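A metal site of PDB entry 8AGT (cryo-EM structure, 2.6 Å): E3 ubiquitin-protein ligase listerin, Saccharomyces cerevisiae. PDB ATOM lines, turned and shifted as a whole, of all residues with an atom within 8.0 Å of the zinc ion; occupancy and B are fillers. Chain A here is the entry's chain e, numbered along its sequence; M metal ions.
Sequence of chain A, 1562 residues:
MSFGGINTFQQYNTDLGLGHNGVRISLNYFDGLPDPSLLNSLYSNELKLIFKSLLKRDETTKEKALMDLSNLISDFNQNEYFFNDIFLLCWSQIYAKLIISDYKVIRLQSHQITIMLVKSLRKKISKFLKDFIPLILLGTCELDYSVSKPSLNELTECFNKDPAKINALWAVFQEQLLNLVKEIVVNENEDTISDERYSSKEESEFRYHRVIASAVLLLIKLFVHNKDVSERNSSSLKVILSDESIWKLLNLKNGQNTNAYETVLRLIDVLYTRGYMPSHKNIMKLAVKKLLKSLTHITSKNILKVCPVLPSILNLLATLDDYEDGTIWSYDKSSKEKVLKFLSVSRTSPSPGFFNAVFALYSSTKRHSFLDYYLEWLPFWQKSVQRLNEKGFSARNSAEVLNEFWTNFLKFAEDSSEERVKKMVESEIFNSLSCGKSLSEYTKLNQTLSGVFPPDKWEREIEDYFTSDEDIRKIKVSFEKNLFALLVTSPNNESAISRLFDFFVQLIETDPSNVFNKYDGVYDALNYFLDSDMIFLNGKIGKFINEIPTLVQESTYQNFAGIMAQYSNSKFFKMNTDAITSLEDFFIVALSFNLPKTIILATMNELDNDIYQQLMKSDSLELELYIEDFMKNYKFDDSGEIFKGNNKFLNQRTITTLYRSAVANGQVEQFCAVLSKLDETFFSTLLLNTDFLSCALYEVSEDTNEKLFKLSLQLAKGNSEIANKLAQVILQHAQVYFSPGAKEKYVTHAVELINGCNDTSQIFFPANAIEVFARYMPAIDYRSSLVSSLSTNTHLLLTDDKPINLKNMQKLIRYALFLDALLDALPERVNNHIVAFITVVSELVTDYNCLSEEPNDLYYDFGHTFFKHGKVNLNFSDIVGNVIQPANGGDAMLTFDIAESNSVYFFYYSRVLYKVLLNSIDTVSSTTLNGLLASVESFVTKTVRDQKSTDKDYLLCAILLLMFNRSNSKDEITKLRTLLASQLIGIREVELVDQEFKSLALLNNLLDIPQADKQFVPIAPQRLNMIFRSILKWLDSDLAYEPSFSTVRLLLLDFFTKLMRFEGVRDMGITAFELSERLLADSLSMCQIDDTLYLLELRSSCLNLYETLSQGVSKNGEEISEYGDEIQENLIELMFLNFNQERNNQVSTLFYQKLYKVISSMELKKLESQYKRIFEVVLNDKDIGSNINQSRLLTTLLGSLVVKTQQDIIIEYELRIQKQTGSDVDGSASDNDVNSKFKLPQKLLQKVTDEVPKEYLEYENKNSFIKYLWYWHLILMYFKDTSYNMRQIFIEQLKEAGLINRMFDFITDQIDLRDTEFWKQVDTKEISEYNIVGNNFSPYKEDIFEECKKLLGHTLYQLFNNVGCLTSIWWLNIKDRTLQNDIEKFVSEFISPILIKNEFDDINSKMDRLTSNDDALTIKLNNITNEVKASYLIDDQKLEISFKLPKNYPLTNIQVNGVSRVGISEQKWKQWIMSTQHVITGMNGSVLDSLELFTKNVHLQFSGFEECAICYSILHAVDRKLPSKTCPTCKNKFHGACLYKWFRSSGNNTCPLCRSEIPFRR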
ATOM      1  N   THR A1526     -14.790  21.818 -35.458  1.00  0.00           N
ATOM      2  CA  THR A1526     -14.793  20.366 -35.354  1.00  0.00           C
ATOM      3  C   THR A1526     -13.959  19.922 -34.166  1.00  0.00           C
ATOM      4  O   THR A1526     -12.837  20.386 -34.006  1.00  0.00           O
ATOM      5  CB  THR A1526     -14.249  19.693 -36.622  1.00  0.00           C
ATOM      6  OG1 THR A1526     -12.983  20.281 -36.964  1.00  0.00           O
ATOM      7  CG2 THR A1526     -15.207  19.856 -37.788  1.00  0.00           C
ATOM      8  N   CYS A1527     -14.498  19.041 -33.343  1.00  0.00           N
ATOM      9  CA  CYS A1527     -13.727  18.503 -32.237  1.00  0.00           C
ATOM     10  C   CYS A1527     -12.611  17.641 -32.807  1.00  0.00           C
ATOM     11  O   CYS A1527     -12.829  16.878 -33.744  1.00  0.00           O
ATOM     12  CB  CYS A1527     -14.621  17.669 -31.331  1.00  0.00           C
ATOM     13  SG  CYS A1527     -13.808  16.794 -29.987  1.00  0.00           S
ATOM     14  N   PRO A1528     -11.391  17.755 -32.261  1.00  0.00           N
ATOM     15  CA  PRO A1528     -10.345  16.858 -32.746  1.00  0.00           C
ATOM     16  C   PRO A1528     -10.683  15.406 -32.465  1.00  0.00           C
ATOM     17  O   PRO A1528     -10.497  14.550 -33.334  1.00  0.00           O
ATOM     18  CB  PRO A1528      -9.110  17.286 -31.937  1.00  0.00           C
ATOM     19  CG  PRO A1528      -9.396  18.695 -31.510  1.00  0.00           C
ATOM     20  CD  PRO A1528     -10.873  18.755 -31.296  1.00  0.00           C
ATOM     21  N   THR A1529     -11.163  15.121 -31.253  1.00  0.00           N
ATOM     22  CA  THR A1529     -11.514  13.751 -30.888  1.00  0.00           C
ATOM     23  C   THR A1529     -12.673  13.164 -31.684  1.00  0.00           C
ATOM     24  O   THR A1529     -12.626  12.006 -32.091  1.00  0.00           O
ATOM     25  CB  THR A1529     -11.831  13.653 -29.383  1.00  0.00           C
ATOM     26  OG1 THR A1529     -10.982  14.554 -28.656  1.00  0.00           O
ATOM     27  CG2 THR A1529     -11.623  12.241 -28.875  1.00  0.00           C
ATOM     28  N   CYS A1530     -13.719  13.960 -31.924  1.00  0.00           N
ATOM     29  CA  CYS A1530     -14.902  13.424 -32.612  1.00  0.00           C
ATOM     30  C   CYS A1530     -15.284  14.140 -33.903  1.00  0.00           C
ATOM     31  O   CYS A1530     -15.268  15.373 -33.973  1.00  0.00           O
ATOM     32  CB  CYS A1530     -16.091  13.302 -31.660  1.00  0.00           C
ATOM     33  SG  CYS A1530     -16.715  14.832 -30.931  1.00  0.00           S
ATOM     34  N   LYS A1531     -15.655  13.372 -34.919  1.00  0.00           N
ATOM     35  CA  LYS A1531     -16.019  13.941 -36.221  1.00  0.00           C
ATOM     36  C   LYS A1531     -17.225  14.860 -36.214  1.00  0.00           C
ATOM     37  O   LYS A1531     -17.291  15.808 -36.999  1.00  0.00           O
ATOM     38  CB  LYS A1531     -16.237  12.833 -37.250  1.00  0.00           C
ATOM     39  CG  LYS A1531     -15.020  11.954 -37.487  1.00  0.00           C
ATOM     40  CD  LYS A1531     -15.337  10.873 -38.504  1.00  0.00           C
ATOM     41  CE  LYS A1531     -14.159   9.933 -38.706  1.00  0.00           C
ATOM     42  NZ  LYS A1531     -14.490   8.841 -39.658  1.00  0.00           N
ATOM     43  N   ASN A1532     -18.195  14.599 -35.339  1.00  0.00           N
ATOM     44  CA  ASN A1532     -19.436  15.379 -35.378  1.00  0.00           C
ATOM     45  C   ASN A1532     -19.159  16.868 -35.295  1.00  0.00           C
ATOM     46  O   ASN A1532     -18.362  17.311 -34.470  1.00  0.00           O
ATOM     47  CB  ASN A1532     -20.354  14.946 -34.239  1.00  0.00           C
ATOM     48  CG  ASN A1532     -20.494  13.441 -34.129  1.00  0.00           C
ATOM     49  OD1 ASN A1532     -19.554  12.752 -33.716  1.00  0.00           O
ATOM     50  ND2 ASN A1532     -21.664  12.925 -34.490  1.00  0.00           N
ATOM     51  N   PHE A1534     -19.757  20.863 -34.543  1.00  0.00           N
ATOM     52  CA  PHE A1534     -20.446  21.714 -33.590  1.00  0.00           C
ATOM     53  C   PHE A1534     -20.430  23.144 -34.098  1.00  0.00           C
ATOM     54  O   PHE A1534     -19.403  23.624 -34.566  1.00  0.00           O
ATOM     55  CB  PHE A1534     -19.734  21.696 -32.236  1.00  0.00           C
ATOM     56  CG  PHE A1534     -19.525  20.322 -31.672  1.00  0.00           C
ATOM     57  CD1 PHE A1534     -20.567  19.646 -31.052  1.00  0.00           C
ATOM     58  CD2 PHE A1534     -18.289  19.706 -31.745  1.00  0.00           C
ATOM     59  CE1 PHE A1534     -20.370  18.390 -30.528  1.00  0.00           C
ATOM     60  CE2 PHE A1534     -18.087  18.443 -31.233  1.00  0.00           C
ATOM     61  CZ  PHE A1534     -19.133  17.781 -30.614  1.00  0.00           C
ATOM     62  N   LEU A1539     -20.754  25.651 -29.512  1.00  0.00           N
ATOM     63  CA  LEU A1539     -19.565  25.152 -28.844  1.00  0.00           C
ATOM     64  C   LEU A1539     -19.068  26.108 -27.768  1.00  0.00           C
ATOM     65  O   LEU A1539     -18.715  25.694 -26.675  1.00  0.00           O
ATOM     66  CB  LEU A1539     -18.466  24.909 -29.866  1.00  0.00           C
ATOM     67  CG  LEU A1539     -17.389  23.901 -29.488  1.00  0.00           C
ATOM     68  CD1 LEU A1539     -18.030  22.629 -28.948  1.00  0.00           C
ATOM     69  CD2 LEU A1539     -16.485  23.598 -30.668  1.00  0.00           C
ATOM     70  N   THR A1550     -14.357  22.405 -23.133  1.00  0.00           N
ATOM     71  CA  THR A1550     -14.713  20.983 -23.078  1.00  0.00           C
ATOM     72  C   THR A1550     -15.673  20.566 -24.178  1.00  0.00           C
ATOM     73  O   THR A1550     -16.661  21.245 -24.432  1.00  0.00           O
ATOM     74  CB  THR A1550     -15.356  20.622 -21.729  1.00  0.00           C
ATOM     75  OG1 THR A1550     -16.548  21.405 -21.543  1.00  0.00           O
ATOM     76  CG2 THR A1550     -14.395  20.896 -20.578  1.00  0.00           C
ATOM     77  N   CYS A1551     -15.387  19.448 -24.847  1.00  0.00           N
ATOM     78  CA  CYS A1551     -16.312  18.933 -25.866  1.00  0.00           C
ATOM     79  C   CYS A1551     -17.594  18.426 -25.224  1.00  0.00           C
ATOM     80  O   CYS A1551     -17.547  17.730 -24.211  1.00  0.00           O
ATOM     81  CB  CYS A1551     -15.646  17.803 -26.649  1.00  0.00           C
ATOM     82  SG  CYS A1551     -16.667  17.038 -27.926  1.00  0.00           S
ATOM     83  N   PRO A1552     -18.759  18.782 -25.793  1.00  0.00           N
ATOM     84  CA  PRO A1552     -20.004  18.220 -25.254  1.00  0.00           C
ATOM     85  C   PRO A1552     -20.099  16.721 -25.435  1.00  0.00           C
ATOM     86  O   PRO A1552     -20.459  16.010 -24.490  1.00  0.00           O
ATOM     87  CB  PRO A1552     -21.087  18.898 -26.097  1.00  0.00           C
ATOM     88  CG  PRO A1552     -20.426  20.082 -26.723  1.00  0.00           C
ATOM     89  CD  PRO A1552     -18.994  19.725 -26.898  1.00  0.00           C
ATOM     90  N   LEU A1553     -19.771  16.226 -26.616  1.00  0.00           N
ATOM     91  CA  LEU A1553     -19.842  14.789 -26.892  1.00  0.00           C
ATOM     92  C   LEU A1553     -18.840  13.934 -26.143  1.00  0.00           C
ATOM     93  O   LEU A1553     -19.180  12.846 -25.684  1.00  0.00           O
ATOM     94  CB  LEU A1553     -19.714  14.520 -28.390  1.00  0.00           C
ATOM     95  CG  LEU A1553     -20.973  14.786 -29.208  1.00  0.00           C
ATOM     96  CD1 LEU A1553     -20.862  14.045 -30.530  1.00  0.00           C
ATOM     97  CD2 LEU A1553     -22.210  14.325 -28.454  1.00  0.00           C
ATOM     98  N   CYS A1554     -17.611  14.409 -26.009  1.00  0.00           N
ATOM     99  CA  CYS A1554     -16.583  13.582 -25.403  1.00  0.00           C
ATOM    100  C   CYS A1554     -15.846  14.245 -24.256  1.00  0.00           C
ATOM    101  O   CYS A1554     -15.784  15.471 -24.174  1.00  0.00           O
ATOM    102  CB  CYS A1554     -15.584  13.103 -26.461  1.00  0.00           C
ATOM    103  SG  CYS A1554     -14.505  14.395 -27.139  1.00  0.00           S
ATOM    104  N   ARG A1555     -15.278  13.441 -23.368  1.00  0.00           N
ATOM    105  CA  ARG A1555     -14.565  13.977 -22.208  1.00  0.00           C
ATOM    106  C   ARG A1555     -13.357  14.806 -22.628  1.00  0.00           C
ATOM    107  O   ARG A1555     -13.054  15.813 -22.001  1.00  0.00           O
ATOM    108  CB  ARG A1555     -14.152  12.856 -21.252  1.00  0.00           C
ATOM    109  CG  ARG A1555     -15.282  12.337 -20.368  1.00  0.00           C
ATOM    110  CD  ARG A1555     -16.181  11.351 -21.094  1.00  0.00           C
ATOM    111  NE  ARG A1555     -17.540  11.369 -20.560  1.00  0.00           N
ATOM    112  CZ  ARG A1555     -18.537  12.091 -21.081  1.00  0.00           C
ATOM    113  NH1 ARG A1555     -18.332  12.852 -22.143  1.00  0.00           N
ATOM    114  NH2 ARG A1555     -19.738  12.045 -20.529  1.00  0.00           N
ATOM    115  N   SER A1556     -12.674  14.375 -23.688  1.00  0.00           N
ATOM    116  CA  SER A1556     -11.478  15.086 -24.114  1.00  0.00           C
ATOM    117  C   SER A1556     -11.763  16.534 -24.498  1.00  0.00           C
ATOM    118  O   SER A1556     -12.756  16.822 -25.167  1.00  0.00           O
ATOM    119  CB  SER A1556     -10.826  14.355 -25.299  1.00  0.00           C
ATOM    120  OG  SER A1556      -9.735  15.092 -25.823  1.00  0.00           O
ATOM    121  N   GLU A1557     -10.888  17.438 -24.087  1.00  0.00           N
ATOM    122  CA  GLU A1557     -11.081  18.867 -24.348  1.00  0.00           C
ATOM    123  C   GLU A1557     -10.839  19.295 -25.791  1.00  0.00           C
ATOM    124  O   GLU A1557     -10.124  18.617 -26.535  1.00  0.00           O
ATOM    125  CB  GLU A1557     -10.196  19.696 -23.413  1.00  0.00           C
ATOM    126  N   ILE A1558     -11.430  20.415 -26.197  1.00  0.00           N
ATOM    127  CA  ILE A1558     -11.198  20.943 -27.541  1.00  0.00           C
ATOM    128  C   ILE A1558     -10.273  22.148 -27.430  1.00  0.00           C
ATOM    129  O   ILE A1558     -10.549  23.078 -26.666  1.00  0.00           O
ATOM    130  CB  ILE A1558     -12.518  21.415 -28.190  1.00  0.00           C
ATOM    131  CG1 ILE A1558     -13.511  20.266 -28.276  1.00  0.00           C
ATOM    132  CG2 ILE A1558     -12.262  21.983 -29.578  1.00  0.00           C
ATOM    133  CD1 ILE A1558     -14.793  20.644 -28.982  1.00  0.00           C
HETATM  134 ZN    ZN M   1     -15.431  15.388 -29.042  1.00  0.00          ZN
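SG of Cys 1554 sits close to O of Ser 1556, at 3.6 Å. The backbone NH (N) of Leu 1553 lies close to the side-chain sulfur (SG) of Cys 1551, at 3.5 Å. The side-chain sulfur (SG) of Cys 1527 sits close to the backbone NH (N) of Thr 1529 (3.4 Å).
Within 4 Å of the zinc ion: Cys 1527, Cys 1530, Cys 1551 and Cys 1554.
The zinc ion is bound by SG of Cys 1554 (2.3 Å), SG of Cys 1551 (2.3 Å), SG of Cys 1527 (2.3 Å) and SG of Cys 1530 (2.4 Å). The zinc ion has four donor atoms within binding distance.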
